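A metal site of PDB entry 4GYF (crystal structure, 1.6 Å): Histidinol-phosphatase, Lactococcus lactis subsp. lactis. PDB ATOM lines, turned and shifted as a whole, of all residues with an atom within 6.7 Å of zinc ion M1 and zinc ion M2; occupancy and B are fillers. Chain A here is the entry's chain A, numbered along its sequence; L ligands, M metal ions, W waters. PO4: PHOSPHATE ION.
Merely in contact with zinc ion M1: His 42 (3.8 Å).
Of the 21 residues printed, 5 come within 4 Å of zinc ion M1.
Ser 107 touches zinc ion M2 (OG to ZN, 3.9 Å).
Of the 21 residues printed, 4 come within 4 Å of zinc ion M2.
N of His 154 is in hydrogen-bond range of OE1 of Glu 193.
ND1 of His 9 lies within hydrogen-bond range of OE2 of Glu 193 (2.7 Å).
The side-chain carboxylate (OD2) of Asp 228 lies within salt-bridge range of the guanidinium group (NH2) of Arg 197 (3.7 Å).
OE2 of Glu 81 sits close to OG of Ser 107 (2.9 Å).
The side-chain carboxylate (OD2) of Asp 228 lies within hydrogen-bond range of the side-chain amide nitrogen (ND2) of Asn 195, at 3.0 Å.
The backbone carbonyl oxygen (O) of Asp 228 sits at hydrogen-bond distance from a ring nitrogen (ND1) of His 230.
A ring nitrogen (ND1) of His 42 sits close to the side-chain carboxylate of Glu 81 (3.3 Å).
The backbone carbonyl oxygen (O) of Thr 40 sits close to a ring nitrogen (ND1) of His 11 (3.3 Å).
Zinc ion M2 is bound by the side-chain carboxylate (OE2) of Glu 81 (2.0 Å), a ring nitrogen (NE2) of His 109 (2.1 Å), a ring nitrogen (NE2) of His 154 (2.1 Å), water W1 (2.1 Å) and an oxygen (O3) of the ligand (2.2 Å).
Zinc ion M1 is bound by O1 of the ligand (1.9 Å), water W1 (2.1 Å), NE2 of His 9 (2.1 Å), NE2 of His 11 (2.2 Å), OE1 of Glu 81 (2.2 Å) and OD1 of Asp 228 (2.2 Å).
Zinc ion M1 has six donor atoms within binding distance.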
ATOM      1  N   HIS A   9      22.206 -24.018 -19.631  1.00  0.00           N
ATOM      2  CA  HIS A   9      21.050 -23.172 -19.296  1.00  0.00           C
ATOM      3  C   HIS A   9      19.817 -23.657 -20.017  1.00  0.00           C
ATOM      4  O   HIS A   9      19.681 -23.432 -21.222  1.00  0.00           O
ATOM      5  CB  HIS A   9      21.317 -21.701 -19.662  1.00  0.00           C
ATOM      6  CG  HIS A   9      20.300 -20.756 -19.103  1.00  0.00           C
ATOM      7  ND1 HIS A   9      20.595 -19.433 -18.832  1.00  0.00           N
ATOM      8  CD2 HIS A   9      19.002 -20.922 -18.756  1.00  0.00           C
ATOM      9  CE1 HIS A   9      19.528 -18.831 -18.342  1.00  0.00           C
ATOM     10  NE2 HIS A   9      18.536 -19.705 -18.304  1.00  0.00           N
ATOM     11  N   PHE A  10      18.900 -24.285 -19.287  1.00  0.00           N
ATOM     12  CA  PHE A  10      17.639 -24.703 -19.908  1.00  0.00           C
ATOM     13  C   PHE A  10      16.634 -25.093 -18.838  1.00  0.00           C
ATOM     14  O   PHE A  10      16.992 -25.278 -17.671  1.00  0.00           O
ATOM     15  CB  PHE A  10      17.848 -25.830 -20.928  1.00  0.00           C
ATOM     16  CG  PHE A  10      18.447 -27.079 -20.356  1.00  0.00           C
ATOM     17  CD1 PHE A  10      17.637 -28.116 -19.903  1.00  0.00           C
ATOM     18  CD2 PHE A  10      19.831 -27.242 -20.314  1.00  0.00           C
ATOM     19  CE1 PHE A  10      18.192 -29.274 -19.379  1.00  0.00           C
ATOM     20  CE2 PHE A  10      20.392 -28.401 -19.811  1.00  0.00           C
ATOM     21  CZ  PHE A  10      19.569 -29.425 -19.335  1.00  0.00           C
ATOM     22  N   HIS A  11      15.371 -25.195 -19.238  1.00  0.00           N
ATOM     23  CA  HIS A  11      14.269 -25.286 -18.281  1.00  0.00           C
ATOM     24  C   HIS A  11      13.321 -26.416 -18.650  1.00  0.00           C
ATOM     25  O   HIS A  11      13.086 -26.668 -19.830  1.00  0.00           O
ATOM     26  CB  HIS A  11      13.470 -23.968 -18.257  1.00  0.00           C
ATOM     27  CG  HIS A  11      14.285 -22.783 -17.865  1.00  0.00           C
ATOM     28  ND1 HIS A  11      14.291 -22.291 -16.575  1.00  0.00           N
ATOM     29  CD2 HIS A  11      15.120 -22.005 -18.581  1.00  0.00           C
ATOM     30  CE1 HIS A  11      15.115 -21.252 -16.516  1.00  0.00           C
ATOM     31  NE2 HIS A  11      15.625 -21.055 -17.716  1.00  0.00           N
ATOM     32  N   ASP A  17       7.479 -21.428 -16.042  1.00  0.00           N
ATOM     33  CA  ASP A  17       7.178 -21.039 -17.427  1.00  0.00           C
ATOM     34  C   ASP A  17       7.623 -22.078 -18.465  1.00  0.00           C
ATOM     35  O   ASP A  17       7.812 -21.751 -19.648  1.00  0.00           O
ATOM     36  CB  ASP A  17       7.823 -19.683 -17.738  1.00  0.00           C
ATOM     37  CG  ASP A  17       9.352 -19.726 -17.706  1.00  0.00           C
ATOM     38  OD1 ASP A  17       9.896 -20.742 -17.251  1.00  0.00           O
ATOM     39  OD2 ASP A  17      10.008 -18.743 -18.126  1.00  0.00           O
ATOM     40  N   THR A  40      18.738 -25.858 -15.225  1.00  0.00           N
ATOM     41  CA  THR A  40      18.827 -24.610 -14.472  1.00  0.00           C
ATOM     42  C   THR A  40      17.429 -24.024 -14.269  1.00  0.00           C
ATOM     43  O   THR A  40      17.056 -23.039 -14.929  1.00  0.00           O
ATOM     44  CB  THR A  40      19.751 -23.562 -15.145  1.00  0.00           C
ATOM     45  OG1 THR A  40      19.275 -23.263 -16.464  1.00  0.00           O
ATOM     46  CG2 THR A  40      21.205 -24.062 -15.250  1.00  0.00           C
ATOM     47  N   HIS A  42      14.016 -22.195 -12.778  1.00  0.00           N
ATOM     48  CA  HIS A  42      13.787 -20.864 -12.206  1.00  0.00           C
ATOM     49  C   HIS A  42      13.437 -20.898 -10.728  1.00  0.00           C
ATOM     50  O   HIS A  42      12.568 -21.671 -10.298  1.00  0.00           O
ATOM     51  CB  HIS A  42      12.585 -20.198 -12.872  1.00  0.00           C
ATOM     52  CG  HIS A  42      12.809 -19.676 -14.254  1.00  0.00           C
ATOM     53  ND1 HIS A  42      13.736 -18.694 -14.549  1.00  0.00           N
ATOM     54  CD2 HIS A  42      12.154 -19.930 -15.411  1.00  0.00           C
ATOM     55  CE1 HIS A  42      13.656 -18.392 -15.841  1.00  0.00           C
ATOM     56  NE2 HIS A  42      12.704 -19.136 -16.381  1.00  0.00           N
ATOM     57  N   GLU A  81      18.567 -21.313 -11.960  1.00  0.00           N
ATOM     58  CA  GLU A  81      18.616 -19.925 -12.401  1.00  0.00           C
ATOM     59  C   GLU A  81      17.913 -19.084 -11.373  1.00  0.00           C
ATOM     60  O   GLU A  81      16.688 -19.112 -11.250  1.00  0.00           O
ATOM     61  CB  GLU A  81      17.958 -19.701 -13.767  1.00  0.00           C
ATOM     62  CG  GLU A  81      18.154 -18.231 -14.235  1.00  0.00           C
ATOM     63  CD  GLU A  81      17.397 -17.858 -15.508  1.00  0.00           C
ATOM     64  OE1 GLU A  81      16.686 -18.713 -16.083  1.00  0.00           O
ATOM     65  OE2 GLU A  81      17.504 -16.690 -15.938  1.00  0.00           O
ATOM     66  N   ILE A 105      23.097 -19.742 -11.776  1.00  0.00           N
ATOM     67  CA  ILE A 105      23.144 -18.553 -12.629  1.00  0.00           C
ATOM     68  C   ILE A 105      22.450 -17.426 -11.875  1.00  0.00           C
ATOM     69  O   ILE A 105      21.358 -17.630 -11.344  1.00  0.00           O
ATOM     70  CB  ILE A 105      22.352 -18.785 -13.924  1.00  0.00           C
ATOM     71  CG1 ILE A 105      22.973 -19.919 -14.751  1.00  0.00           C
ATOM     72  CG2 ILE A 105      22.265 -17.500 -14.751  1.00  0.00           C
ATOM     73  CD1 ILE A 105      22.094 -20.348 -15.925  1.00  0.00           C
ATOM     74  N   SER A 107      20.549 -13.952 -12.405  1.00  0.00           N
ATOM     75  CA  SER A 107      19.892 -13.226 -13.484  1.00  0.00           C
ATOM     76  C   SER A 107      19.080 -12.061 -12.943  1.00  0.00           C
ATOM     77  O   SER A 107      18.622 -12.088 -11.793  1.00  0.00           O
ATOM     78  CB  SER A 107      18.953 -14.172 -14.224  1.00  0.00           C
ATOM     79  OG  SER A 107      19.691 -15.120 -14.961  1.00  0.00           O
ATOM     80  N   VAL A 108      18.877 -11.052 -13.786  1.00  0.00           N
ATOM     81  CA  VAL A 108      17.953  -9.982 -13.445  1.00  0.00           C
ATOM     82  C   VAL A 108      16.732 -10.100 -14.355  1.00  0.00           C
ATOM     83  O   VAL A 108      16.854 -10.037 -15.584  1.00  0.00           O
ATOM     84  CB  VAL A 108      18.589  -8.594 -13.589  1.00  0.00           C
ATOM     85  CG1 VAL A 108      17.540  -7.487 -13.372  1.00  0.00           C
ATOM     86  CG2 VAL A 108      19.708  -8.421 -12.586  1.00  0.00           C
ATOM     87  N   HIS A 109      15.569 -10.282 -13.724  1.00  0.00           N
ATOM     88  CA  HIS A 109      14.295 -10.445 -14.438  1.00  0.00           C
ATOM     89  C   HIS A 109      13.282  -9.363 -14.101  1.00  0.00           C
ATOM     90  O   HIS A 109      12.314  -9.153 -14.848  1.00  0.00           O
ATOM     91  CB  HIS A 109      13.685 -11.808 -14.104  1.00  0.00           C
ATOM     92  CG  HIS A 109      14.471 -12.978 -14.620  1.00  0.00           C
ATOM     93  ND1 HIS A 109      14.639 -14.126 -13.885  1.00  0.00           N
ATOM     94  CD2 HIS A 109      15.117 -13.173 -15.799  1.00  0.00           C
ATOM     95  CE1 HIS A 109      15.360 -14.996 -14.597  1.00  0.00           C
ATOM     96  NE2 HIS A 109      15.657 -14.442 -15.754  1.00  0.00           N
ATOM     97  N   GLY A 153      23.844 -14.427 -15.825  1.00  0.00           N
ATOM     98  CA  GLY A 153      22.980 -14.764 -16.939  1.00  0.00           C
ATOM     99  C   GLY A 153      22.616 -13.642 -17.894  1.00  0.00           C
ATOM    100  O   GLY A 153      22.520 -12.464 -17.508  1.00  0.00           O
ATOM    101  N   HIS A 154      22.393 -14.026 -19.148  1.00  0.00           N
ATOM    102  CA  HIS A 154      21.902 -13.143 -20.220  1.00  0.00           C
ATOM    103  C   HIS A 154      21.996 -11.625 -20.051  1.00  0.00           C
ATOM    104  O   HIS A 154      20.991 -10.970 -19.770  1.00  0.00           O
ATOM    105  CB  HIS A 154      20.468 -13.550 -20.627  1.00  0.00           C
ATOM    106  CG  HIS A 154      19.512 -13.720 -19.472  1.00  0.00           C
ATOM    107  ND1 HIS A 154      19.357 -12.795 -18.465  1.00  0.00           N
ATOM    108  CD2 HIS A 154      18.620 -14.705 -19.218  1.00  0.00           C
ATOM    109  CE1 HIS A 154      18.418 -13.211 -17.622  1.00  0.00           C
ATOM    110  NE2 HIS A 154      17.953 -14.366 -18.064  1.00  0.00           N
ATOM    111  N   TYR A 157      19.385  -9.649 -21.919  1.00  0.00           N
ATOM    112  CA  TYR A 157      17.979  -9.953 -21.621  1.00  0.00           C
ATOM    113  C   TYR A 157      17.041  -8.815 -22.030  1.00  0.00           C
ATOM    114  O   TYR A 157      15.966  -9.046 -22.598  1.00  0.00           O
ATOM    115  CB  TYR A 157      17.828 -10.246 -20.121  1.00  0.00           C
ATOM    116  CG  TYR A 157      16.468 -10.727 -19.664  1.00  0.00           C
ATOM    117  CD1 TYR A 157      16.118 -12.067 -19.755  1.00  0.00           C
ATOM    118  CD2 TYR A 157      15.568  -9.847 -19.081  1.00  0.00           C
ATOM    119  CE1 TYR A 157      14.879 -12.515 -19.287  1.00  0.00           C
ATOM    120  CE2 TYR A 157      14.336 -10.279 -18.631  1.00  0.00           C
ATOM    121  CZ  TYR A 157      14.000 -11.615 -18.741  1.00  0.00           C
ATOM    122  OH  TYR A 157      12.771 -12.038 -18.281  1.00  0.00           O
ATOM    123  N   ARG A 160      15.537  -8.654 -25.531  1.00  0.00           N
ATOM    124  CA  ARG A 160      14.561  -9.638 -26.005  1.00  0.00           C
ATOM    125  C   ARG A 160      13.190  -9.018 -26.172  1.00  0.00           C
ATOM    126  O   ARG A 160      12.342  -9.507 -26.956  1.00  0.00           O
ATOM    127  CB  ARG A 160      14.452 -10.798 -25.012  1.00  0.00           C
ATOM    128  CG  ARG A 160      15.740 -11.572 -24.758  1.00  0.00           C
ATOM    129  CD  ARG A 160      15.483 -12.526 -23.605  1.00  0.00           C
ATOM    130  NE  ARG A 160      16.546 -13.504 -23.440  1.00  0.00           N
ATOM    131  CZ  ARG A 160      16.446 -14.563 -22.648  1.00  0.00           C
ATOM    132  NH1 ARG A 160      15.331 -14.783 -21.970  1.00  0.00           N
ATOM    133  NH2 ARG A 160      17.461 -15.416 -22.552  1.00  0.00           N
ATOM    134  N   GLU A 193      27.916 -15.737 -18.822  1.00  0.00           N
ATOM    135  CA  GLU A 193      27.122 -16.631 -19.661  1.00  0.00           C
ATOM    136  C   GLU A 193      27.004 -16.133 -21.092  1.00  0.00           C
ATOM    137  O   GLU A 193      26.666 -14.973 -21.321  1.00  0.00           O
ATOM    138  CB  GLU A 193      25.718 -16.804 -19.092  1.00  0.00           C
ATOM    139  CG  GLU A 193      24.806 -17.561 -20.032  1.00  0.00           C
ATOM    140  CD  GLU A 193      23.417 -17.758 -19.467  1.00  0.00           C
ATOM    141  OE1 GLU A 193      22.566 -16.853 -19.639  1.00  0.00           O
ATOM    142  OE2 GLU A 193      23.189 -18.830 -18.864  1.00  0.00           O
ATOM    143  N   ASN A 195      24.523 -16.657 -23.816  1.00  0.00           N
ATOM    144  CA  ASN A 195      23.155 -17.154 -23.910  1.00  0.00           C
ATOM    145  C   ASN A 195      22.711 -17.059 -25.354  1.00  0.00           C
ATOM    146  O   ASN A 195      22.758 -15.983 -25.956  1.00  0.00           O
ATOM    147  CB  ASN A 195      22.250 -16.281 -23.022  1.00  0.00           C
ATOM    148  CG  ASN A 195      20.839 -16.828 -22.899  1.00  0.00           C
ATOM    149  OD1 ASN A 195      20.129 -17.010 -23.898  1.00  0.00           O
ATOM    150  ND2 ASN A 195      20.414 -17.080 -21.660  1.00  0.00           N
ATOM    151  N   ARG A 197      19.785 -17.490 -26.883  1.00  0.00           N
ATOM    152  CA  ARG A 197      18.369 -17.213 -27.192  1.00  0.00           C
ATOM    153  C   ARG A 197      18.163 -16.361 -28.445  1.00  0.00           C
ATOM    154  O   ARG A 197      17.351 -16.700 -29.315  1.00  0.00           O
ATOM    155  CB  ARG A 197      17.670 -16.561 -25.997  1.00  0.00           C
ATOM    156  CG  ARG A 197      16.233 -16.080 -26.289  1.00  0.00           C
ATOM    157  CD  ARG A 197      15.237 -17.229 -26.396  1.00  0.00           C
ATOM    158  NE  ARG A 197      15.136 -17.933 -25.127  1.00  0.00           N
ATOM    159  CZ  ARG A 197      14.417 -17.504 -24.088  1.00  0.00           C
ATOM    160  NH1 ARG A 197      13.724 -16.374 -24.194  1.00  0.00           N
ATOM    161  NH2 ARG A 197      14.392 -18.185 -22.953  1.00  0.00           N
ATOM    162  N   ASP A 228      19.077 -21.522 -23.060  1.00  0.00           N
ATOM    163  CA  ASP A 228      17.885 -20.997 -22.396  1.00  0.00           C
ATOM    164  C   ASP A 228      16.608 -21.589 -23.007  1.00  0.00           C
ATOM    165  O   ASP A 228      15.547 -20.972 -22.952  1.00  0.00           O
ATOM    166  CB  ASP A 228      17.825 -19.466 -22.470  1.00  0.00           C
ATOM    167  CG  ASP A 228      17.279 -18.840 -21.202  1.00  0.00           C
ATOM    168  OD1 ASP A 228      16.576 -19.529 -20.411  1.00  0.00           O
ATOM    169  OD2 ASP A 228      17.542 -17.636 -20.998  1.00  0.00           O
ATOM    170  N   SER A 229      16.722 -22.794 -23.559  1.00  0.00           N
ATOM    171  CA  SER A 229      15.546 -23.413 -24.176  1.00  0.00           C
ATOM    172  C   SER A 229      14.559 -23.892 -23.111  1.00  0.00           C
ATOM    173  O   SER A 229      14.954 -24.506 -22.122  1.00  0.00           O
ATOM    174  CB  SER A 229      15.955 -24.585 -25.074  1.00  0.00           C
ATOM    175  OG  SER A 229      14.863 -24.969 -25.898  1.00  0.00           O
ATOM    176  N   HIS A 230      13.276 -23.600 -23.318  1.00  0.00           N
ATOM    177  CA  HIS A 230      12.232 -24.046 -22.403  1.00  0.00           C
ATOM    178  C   HIS A 230      11.522 -25.272 -22.993  1.00  0.00           C
ATOM    179  O   HIS A 230      10.584 -25.813 -22.398  1.00  0.00           O
ATOM    180  CB  HIS A 230      11.246 -22.912 -22.117  1.00  0.00           C
ATOM    181  CG  HIS A 230      11.805 -21.816 -21.250  1.00  0.00           C
ATOM    182  ND1 HIS A 230      13.012 -21.213 -21.517  1.00  0.00           N
ATOM    183  CD2 HIS A 230      11.333 -21.235 -20.133  1.00  0.00           C
ATOM    184  CE1 HIS A 230      13.264 -20.299 -20.595  1.00  0.00           C
ATOM    185  NE2 HIS A 230      12.248 -20.275 -19.742  1.00  0.00           N
HETATM  186  P   PO4 L   1      14.135 -17.063 -19.080  1.00  0.00           P
HETATM  187  O1  PO4 L   1      14.808 -18.340 -18.654  1.00  0.00           O
HETATM  188  O2  PO4 L   1      14.441 -16.717 -20.511  1.00  0.00           O
HETATM  189  O3  PO4 L   1      14.571 -15.935 -18.173  1.00  0.00           O
HETATM  190  O4  PO4 L   1      12.636 -17.268 -18.949  1.00  0.00           O
HETATM  191 ZN    ZN M   1      16.472 -19.134 -18.220  1.00  0.00          ZN
HETATM  192 ZN    ZN M   2      16.499 -15.622 -17.229  1.00  0.00          ZN
HETATM  193 ZN    ZN M   3      11.949 -18.948 -18.222  1.00  0.00          ZN
HETATM  194  O   HOH W   1      17.033 -17.110 -18.621  1.00  0.00           O
